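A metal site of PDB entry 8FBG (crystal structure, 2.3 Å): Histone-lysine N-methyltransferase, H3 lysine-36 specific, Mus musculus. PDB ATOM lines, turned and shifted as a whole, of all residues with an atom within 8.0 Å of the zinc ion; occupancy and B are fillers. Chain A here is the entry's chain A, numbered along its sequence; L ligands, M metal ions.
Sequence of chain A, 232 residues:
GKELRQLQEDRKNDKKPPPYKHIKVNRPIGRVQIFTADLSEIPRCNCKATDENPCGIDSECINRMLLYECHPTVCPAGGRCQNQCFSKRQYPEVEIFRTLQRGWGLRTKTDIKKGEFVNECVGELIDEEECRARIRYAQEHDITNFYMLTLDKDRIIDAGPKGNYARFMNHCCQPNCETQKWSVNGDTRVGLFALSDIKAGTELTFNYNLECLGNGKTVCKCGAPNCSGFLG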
ATOM      1  N   ARG A 102       3.740 -17.644  17.509  1.00  0.00           N
ATOM      2  CA  ARG A 102       3.589 -16.204  17.229  1.00  0.00           C
ATOM      3  C   ARG A 102       3.358 -15.368  18.504  1.00  0.00           C
ATOM      4  O   ARG A 102       2.777 -14.291  18.440  1.00  0.00           O
ATOM      5  CB  ARG A 102       2.448 -15.962  16.221  1.00  0.00           C
ATOM      6  CG  ARG A 102       2.668 -16.594  14.850  1.00  0.00           C
ATOM      7  CD  ARG A 102       1.358 -16.853  14.148  1.00  0.00           C
ATOM      8  NE  ARG A 102       0.564 -17.815  14.901  1.00  0.00           N
ATOM      9  CZ  ARG A 102      -0.681 -17.628  15.289  1.00  0.00           C
ATOM     10  NH1 ARG A 102      -1.339 -16.525  14.932  1.00  0.00           N
ATOM     11  NH2 ARG A 102      -1.295 -18.551  16.010  1.00  0.00           N
ATOM     12  N   HIS A 171      -0.738 -11.441  12.640  1.00  0.00           N
ATOM     13  CA  HIS A 171      -0.870 -11.483  11.201  1.00  0.00           C
ATOM     14  C   HIS A 171      -1.240 -12.941  10.757  1.00  0.00           C
ATOM     15  O   HIS A 171      -0.794 -13.903  11.362  1.00  0.00           O
ATOM     16  CB  HIS A 171       0.455 -11.057  10.511  1.00  0.00           C
ATOM     17  CG  HIS A 171       0.445 -11.354   9.060  1.00  0.00           C
ATOM     18  ND1 HIS A 171      -0.334 -10.614   8.181  1.00  0.00           N
ATOM     19  CD2 HIS A 171       0.972 -12.410   8.386  1.00  0.00           C
ATOM     20  CE1 HIS A 171      -0.208 -11.215   7.013  1.00  0.00           C
ATOM     21  NE2 HIS A 171       0.544 -12.305   7.091  1.00  0.00           N
ATOM     22  N   CYS A 172      -1.966 -13.039   9.644  1.00  0.00           N
ATOM     23  CA  CYS A 172      -2.332 -14.279   8.978  1.00  0.00           C
ATOM     24  C   CYS A 172      -2.542 -14.018   7.484  1.00  0.00           C
ATOM     25  O   CYS A 172      -3.134 -12.997   7.116  1.00  0.00           O
ATOM     26  CB  CYS A 172      -3.577 -14.890   9.611  1.00  0.00           C
ATOM     27  SG  CYS A 172      -3.967 -16.543   9.024  1.00  0.00           S
ATOM     28  N   CYS A 173      -2.068 -14.946   6.648  1.00  0.00           N
ATOM     29  CA  CYS A 173      -2.214 -14.941   5.192  1.00  0.00           C
ATOM     30  C   CYS A 173      -3.646 -15.341   4.795  1.00  0.00           C
ATOM     31  O   CYS A 173      -4.060 -15.086   3.666  1.00  0.00           O
ATOM     32  CB  CYS A 173      -1.182 -15.845   4.541  1.00  0.00           C
ATOM     33  SG  CYS A 173       0.527 -15.315   4.801  1.00  0.00           S
ATOM     34  N   GLN A 174      -4.398 -15.941   5.743  1.00  0.00           N
ATOM     35  CA  GLN A 174      -5.800 -16.349   5.586  1.00  0.00           C
ATOM     36  C   GLN A 174      -6.525 -15.781   6.817  1.00  0.00           C
ATOM     37  O   GLN A 174      -6.883 -16.530   7.741  1.00  0.00           O
ATOM     38  CB  GLN A 174      -5.857 -17.888   5.534  1.00  0.00           C
ATOM     39  CG  GLN A 174      -7.128 -18.441   4.929  1.00  0.00           C
ATOM     40  CD  GLN A 174      -7.068 -19.944   4.984  1.00  0.00           C
ATOM     41  OE1 GLN A 174      -7.196 -20.570   6.065  1.00  0.00           O
ATOM     42  NE2 GLN A 174      -6.847 -20.561   3.823  1.00  0.00           N
ATOM     43  N   ASN A 207      -4.477  -9.449   7.907  1.00  0.00           N
ATOM     44  CA  ASN A 207      -3.320  -9.417   7.026  1.00  0.00           C
ATOM     45  C   ASN A 207      -2.713  -8.068   7.228  1.00  0.00           C
ATOM     46  O   ASN A 207      -3.389  -7.077   6.967  1.00  0.00           O
ATOM     47  CB  ASN A 207      -3.731  -9.618   5.549  1.00  0.00           C
ATOM     48  CG  ASN A 207      -2.607 -10.061   4.658  1.00  0.00           C
ATOM     49  OD1 ASN A 207      -1.509  -9.511   4.653  1.00  0.00           O
ATOM     50  ND2 ASN A 207      -2.878 -11.072   3.857  1.00  0.00           N
ATOM     51  N   VAL A 219       9.806 -14.391   9.906  1.00  0.00           N
ATOM     52  CA  VAL A 219       9.252 -15.554   9.195  1.00  0.00           C
ATOM     53  C   VAL A 219       7.774 -15.744   9.622  1.00  0.00           C
ATOM     54  O   VAL A 219       7.505 -15.857  10.824  1.00  0.00           O
ATOM     55  CB  VAL A 219      10.134 -16.835   9.415  1.00  0.00           C
ATOM     56  CG1 VAL A 219       9.436 -18.118   8.969  1.00  0.00           C
ATOM     57  CG2 VAL A 219      11.490 -16.695   8.727  1.00  0.00           C
ATOM     58  N   CYS A 220       6.833 -15.736   8.648  1.00  0.00           N
ATOM     59  CA  CYS A 220       5.407 -15.897   8.967  1.00  0.00           C
ATOM     60  C   CYS A 220       5.115 -17.289   9.469  1.00  0.00           C
ATOM     61  O   CYS A 220       5.391 -18.263   8.780  1.00  0.00           O
ATOM     62  CB  CYS A 220       4.520 -15.554   7.782  1.00  0.00           C
ATOM     63  SG  CYS A 220       2.751 -15.628   8.166  1.00  0.00           S
ATOM     64  N   LYS A 221       4.522 -17.370  10.668  1.00  0.00           N
ATOM     65  CA  LYS A 221       4.170 -18.633  11.300  1.00  0.00           C
ATOM     66  C   LYS A 221       2.638 -18.793  11.405  1.00  0.00           C
ATOM     67  O   LYS A 221       2.199 -19.547  12.269  1.00  0.00           O
ATOM     68  CB  LYS A 221       4.836 -18.752  12.694  1.00  0.00           C
ATOM     69  CG  LYS A 221       6.382 -18.697  12.716  1.00  0.00           C
ATOM     70  CD  LYS A 221       7.035 -20.026  12.322  1.00  0.00           C
ATOM     71  CE  LYS A 221       8.504 -20.098  12.664  1.00  0.00           C
ATOM     72  NZ  LYS A 221       9.050 -21.480  12.508  1.00  0.00           N
ATOM     73  N   CYS A 222       1.823 -18.117  10.519  1.00  0.00           N
ATOM     74  CA  CYS A 222       0.355 -18.229  10.550  1.00  0.00           C
ATOM     75  C   CYS A 222      -0.118 -19.681  10.287  1.00  0.00           C
ATOM     76  O   CYS A 222      -1.171 -20.067  10.798  1.00  0.00           O
ATOM     77  CB  CYS A 222      -0.339 -17.234   9.608  1.00  0.00           C
ATOM     78  SG  CYS A 222      -0.325 -17.682   7.841  1.00  0.00           S
ATOM     79  N   GLY A 223       0.666 -20.463   9.524  1.00  0.00           N
ATOM     80  CA  GLY A 223       0.398 -21.863   9.239  1.00  0.00           C
ATOM     81  C   GLY A 223      -0.770 -22.127   8.312  1.00  0.00           C
ATOM     82  O   GLY A 223      -1.323 -23.214   8.323  1.00  0.00           O
ATOM     83  N   ALA A 224      -1.148 -21.113   7.513  1.00  0.00           N
ATOM     84  CA  ALA A 224      -2.247 -21.219   6.550  1.00  0.00           C
ATOM     85  C   ALA A 224      -1.759 -22.026   5.329  1.00  0.00           C
ATOM     86  O   ALA A 224      -0.540 -22.113   5.119  1.00  0.00           O
ATOM     87  CB  ALA A 224      -2.682 -19.816   6.132  1.00  0.00           C
ATOM     88  N   PRO A 225      -2.653 -22.654   4.527  1.00  0.00           N
ATOM     89  CA  PRO A 225      -2.165 -23.427   3.372  1.00  0.00           C
ATOM     90  C   PRO A 225      -1.666 -22.554   2.205  1.00  0.00           C
ATOM     91  O   PRO A 225      -0.946 -23.034   1.330  1.00  0.00           O
ATOM     92  CB  PRO A 225      -3.390 -24.266   2.957  1.00  0.00           C
ATOM     93  CG  PRO A 225      -4.559 -23.532   3.454  1.00  0.00           C
ATOM     94  CD  PRO A 225      -4.129 -22.690   4.629  1.00  0.00           C
ATOM     95  N   ASN A 226      -2.050 -21.261   2.214  1.00  0.00           N
ATOM     96  CA  ASN A 226      -1.714 -20.262   1.218  1.00  0.00           C
ATOM     97  C   ASN A 226      -0.674 -19.257   1.760  1.00  0.00           C
ATOM     98  O   ASN A 226      -0.595 -18.148   1.249  1.00  0.00           O
ATOM     99  CB  ASN A 226      -3.000 -19.534   0.810  1.00  0.00           C
ATOM    100  CG  ASN A 226      -3.618 -18.686   1.902  1.00  0.00           C
ATOM    101  OD1 ASN A 226      -3.618 -19.049   3.099  1.00  0.00           O
ATOM    102  ND2 ASN A 226      -4.145 -17.523   1.524  1.00  0.00           N
ATOM    103  N   CYS A 227       0.109 -19.631   2.813  1.00  0.00           N
ATOM    104  CA  CYS A 227       1.094 -18.744   3.431  1.00  0.00           C
ATOM    105  C   CYS A 227       2.226 -18.345   2.453  1.00  0.00           C
ATOM    106  O   CYS A 227       2.826 -19.219   1.854  1.00  0.00           O
ATOM    107  CB  CYS A 227       1.670 -19.363   4.699  1.00  0.00           C
ATOM    108  SG  CYS A 227       2.804 -18.265   5.608  1.00  0.00           S
ATOM    109  N   SER A 228       2.534 -17.046   2.363  1.00  0.00           N
ATOM    110  CA  SER A 228       3.606 -16.509   1.512  1.00  0.00           C
ATOM    111  C   SER A 228       4.999 -16.533   2.220  1.00  0.00           C
ATOM    112  O   SER A 228       6.003 -16.312   1.569  1.00  0.00           O
ATOM    113  CB  SER A 228       3.263 -15.100   1.020  1.00  0.00           C
ATOM    114  OG  SER A 228       3.278 -14.117   2.046  1.00  0.00           O
ATOM    115  N   GLY A 229       5.031 -16.834   3.511  1.00  0.00           N
ATOM    116  CA  GLY A 229       6.248 -16.947   4.305  1.00  0.00           C
ATOM    117  C   GLY A 229       6.682 -15.674   5.017  1.00  0.00           C
ATOM    118  O   GLY A 229       7.527 -15.720   5.922  1.00  0.00           O
ATOM    119  N   PHE A 230       6.086 -14.536   4.623  1.00  0.00           N
ATOM    120  CA  PHE A 230       6.399 -13.208   5.135  1.00  0.00           C
ATOM    121  C   PHE A 230       5.172 -12.539   5.761  1.00  0.00           C
ATOM    122  O   PHE A 230       4.051 -12.824   5.338  1.00  0.00           O
ATOM    123  CB  PHE A 230       6.963 -12.324   4.010  1.00  0.00           C
ATOM    124  CG  PHE A 230       7.934 -13.021   3.095  1.00  0.00           C
ATOM    125  N   LEU A 231       5.402 -11.651   6.752  1.00  0.00           N
ATOM    126  CA  LEU A 231       4.349 -10.886   7.420  1.00  0.00           C
ATOM    127  C   LEU A 231       3.856  -9.806   6.471  1.00  0.00           C
ATOM    128  O   LEU A 231       4.638  -8.976   6.008  1.00  0.00           O
ATOM    129  CB  LEU A 231       4.835 -10.208   8.733  1.00  0.00           C
ATOM    130  CG  LEU A 231       5.262 -11.064   9.920  1.00  0.00           C
ATOM    131  CD1 LEU A 231       5.031 -10.318  11.204  1.00  0.00           C
ATOM    132  CD2 LEU A 231       4.522 -12.354   9.960  1.00  0.00           C
ATOM    133  N   GLY A 232       2.560  -9.864   6.169  1.00  0.00           N
ATOM    134  CA  GLY A 232       1.928  -8.922   5.263  1.00  0.00           C
ATOM    135  C   GLY A 232       2.356  -9.082   3.827  1.00  0.00           C
ATOM    136  O   GLY A 232       1.547  -8.881   2.918  1.00  0.00           O
HETATM  137  N1  LIG L   1       2.356 -11.580  19.039  1.00  0.00           N
HETATM  138  C1  LIG L   1       2.391 -10.205  19.562  1.00  0.00           C
HETATM  139  C2  LIG L   1       2.697 -10.219  21.099  1.00  0.00           C
HETATM  140  O1  LIG L   1       3.085 -11.324  21.529  1.00  0.00           O
HETATM  141  O2  LIG L   1       2.607  -9.164  21.767  1.00  0.00           O
HETATM  142  C3  LIG L   1       1.046  -9.477  19.301  1.00  0.00           C
HETATM  143  C4  LIG L   1       0.921  -8.996  17.816  1.00  0.00           C
HETATM  144  S1  LIG L   1       2.021  -7.629  17.572  1.00  0.00           S
HETATM  145  C5  LIG L   1       0.958  -6.473  16.804  1.00  0.00           C
HETATM  146  C6  LIG L   1       2.902  -8.208  16.133  1.00  0.00           C
HETATM  147  C7  LIG L   1       4.228  -8.935  16.400  1.00  0.00           C
HETATM  148  O3  LIG L   1       3.936 -10.330  16.658  1.00  0.00           O
HETATM  149  C8  LIG L   1       5.172  -8.919  15.193  1.00  0.00           C
HETATM  150  O4  LIG L   1       6.125  -7.868  15.302  1.00  0.00           O
HETATM  151  C9  LIG L   1       5.833 -10.303  15.248  1.00  0.00           C
HETATM  152  O5  LIG L   1       6.976 -10.314  16.096  1.00  0.00           O
HETATM  153  C10 LIG L   1       4.710 -11.166  15.835  1.00  0.00           C
HETATM  154  N2  LIG L   1       3.843 -11.814  14.848  1.00  0.00           N
HETATM  155  C11 LIG L   1       2.557 -11.437  14.519  1.00  0.00           C
HETATM  156  N3  LIG L   1       2.007 -12.176  13.593  1.00  0.00           N
HETATM  157  C12 LIG L   1       2.995 -13.109  13.284  1.00  0.00           C
HETATM  158  C13 LIG L   1       3.066 -14.121  12.302  1.00  0.00           C
HETATM  159  N4  LIG L   1       2.086 -14.385  11.444  1.00  0.00           N
HETATM  160  N5  LIG L   1       4.222 -14.828  12.210  1.00  0.00           N
HETATM  161  C14 LIG L   1       5.220 -14.536  13.055  1.00  0.00           C
HETATM  162  N6  LIG L   1       5.266 -13.617  14.022  1.00  0.00           N
HETATM  163  C15 LIG L   1       4.117 -12.909  14.068  1.00  0.00           C
HETATM  164 ZN    ZN M   1       1.418 -16.718   6.663  1.00  0.00          ZN
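A nitrogen (N1) of the ligand sits at hydrogen-bond distance from the backbone carbonyl oxygen (O) of Arg 102 (2.8 Å).
N of His 171 lies within hydrogen-bond range of N3 of the ligand.
The side-chain sulfur (SG) of Cys 220 lies close to a nitrogen (N4) of the ligand.
A nitrogen (N5) of the ligand lies within hydrogen-bond range of the backbone NH (N) of Lys 221 (3.0 Å).
The backbone carbonyl oxygen (O) of His 171 is in hydrogen-bond range of a nitrogen (N4) of the ligand (2.9 Å).
The backbone NH (N) of Gly 229 sits close to the side-chain sulfur (SG) of Cys 227 (3.4 Å).
NE2 of His 171 sits close to SG of Cys 173 (3.8 Å).
The backbone NH (N) of Cys 220 lies within hydrogen-bond range of the backbone carbonyl oxygen (O) of Gly 229, at 2.8 Å.
The backbone carbonyl oxygen (O) of Cys 173 sits at hydrogen-bond distance from the side-chain amide nitrogen (ND2) of Asn 226 (3.2 Å).
The backbone NH (N) of Ser 228 lies close to the side-chain sulfur (SG) of Cys 173.
SG of Cys 222 sits close to N of Ala 224.
The zinc ion is bound by the side-chain sulfur of Cys 220 (2.3 Å), the side-chain sulfur of Cys 222 (2.3 Å), the side-chain sulfur of Cys 227 (2.3 Å) and the side-chain sulfur of Cys 173 (2.5 Å).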
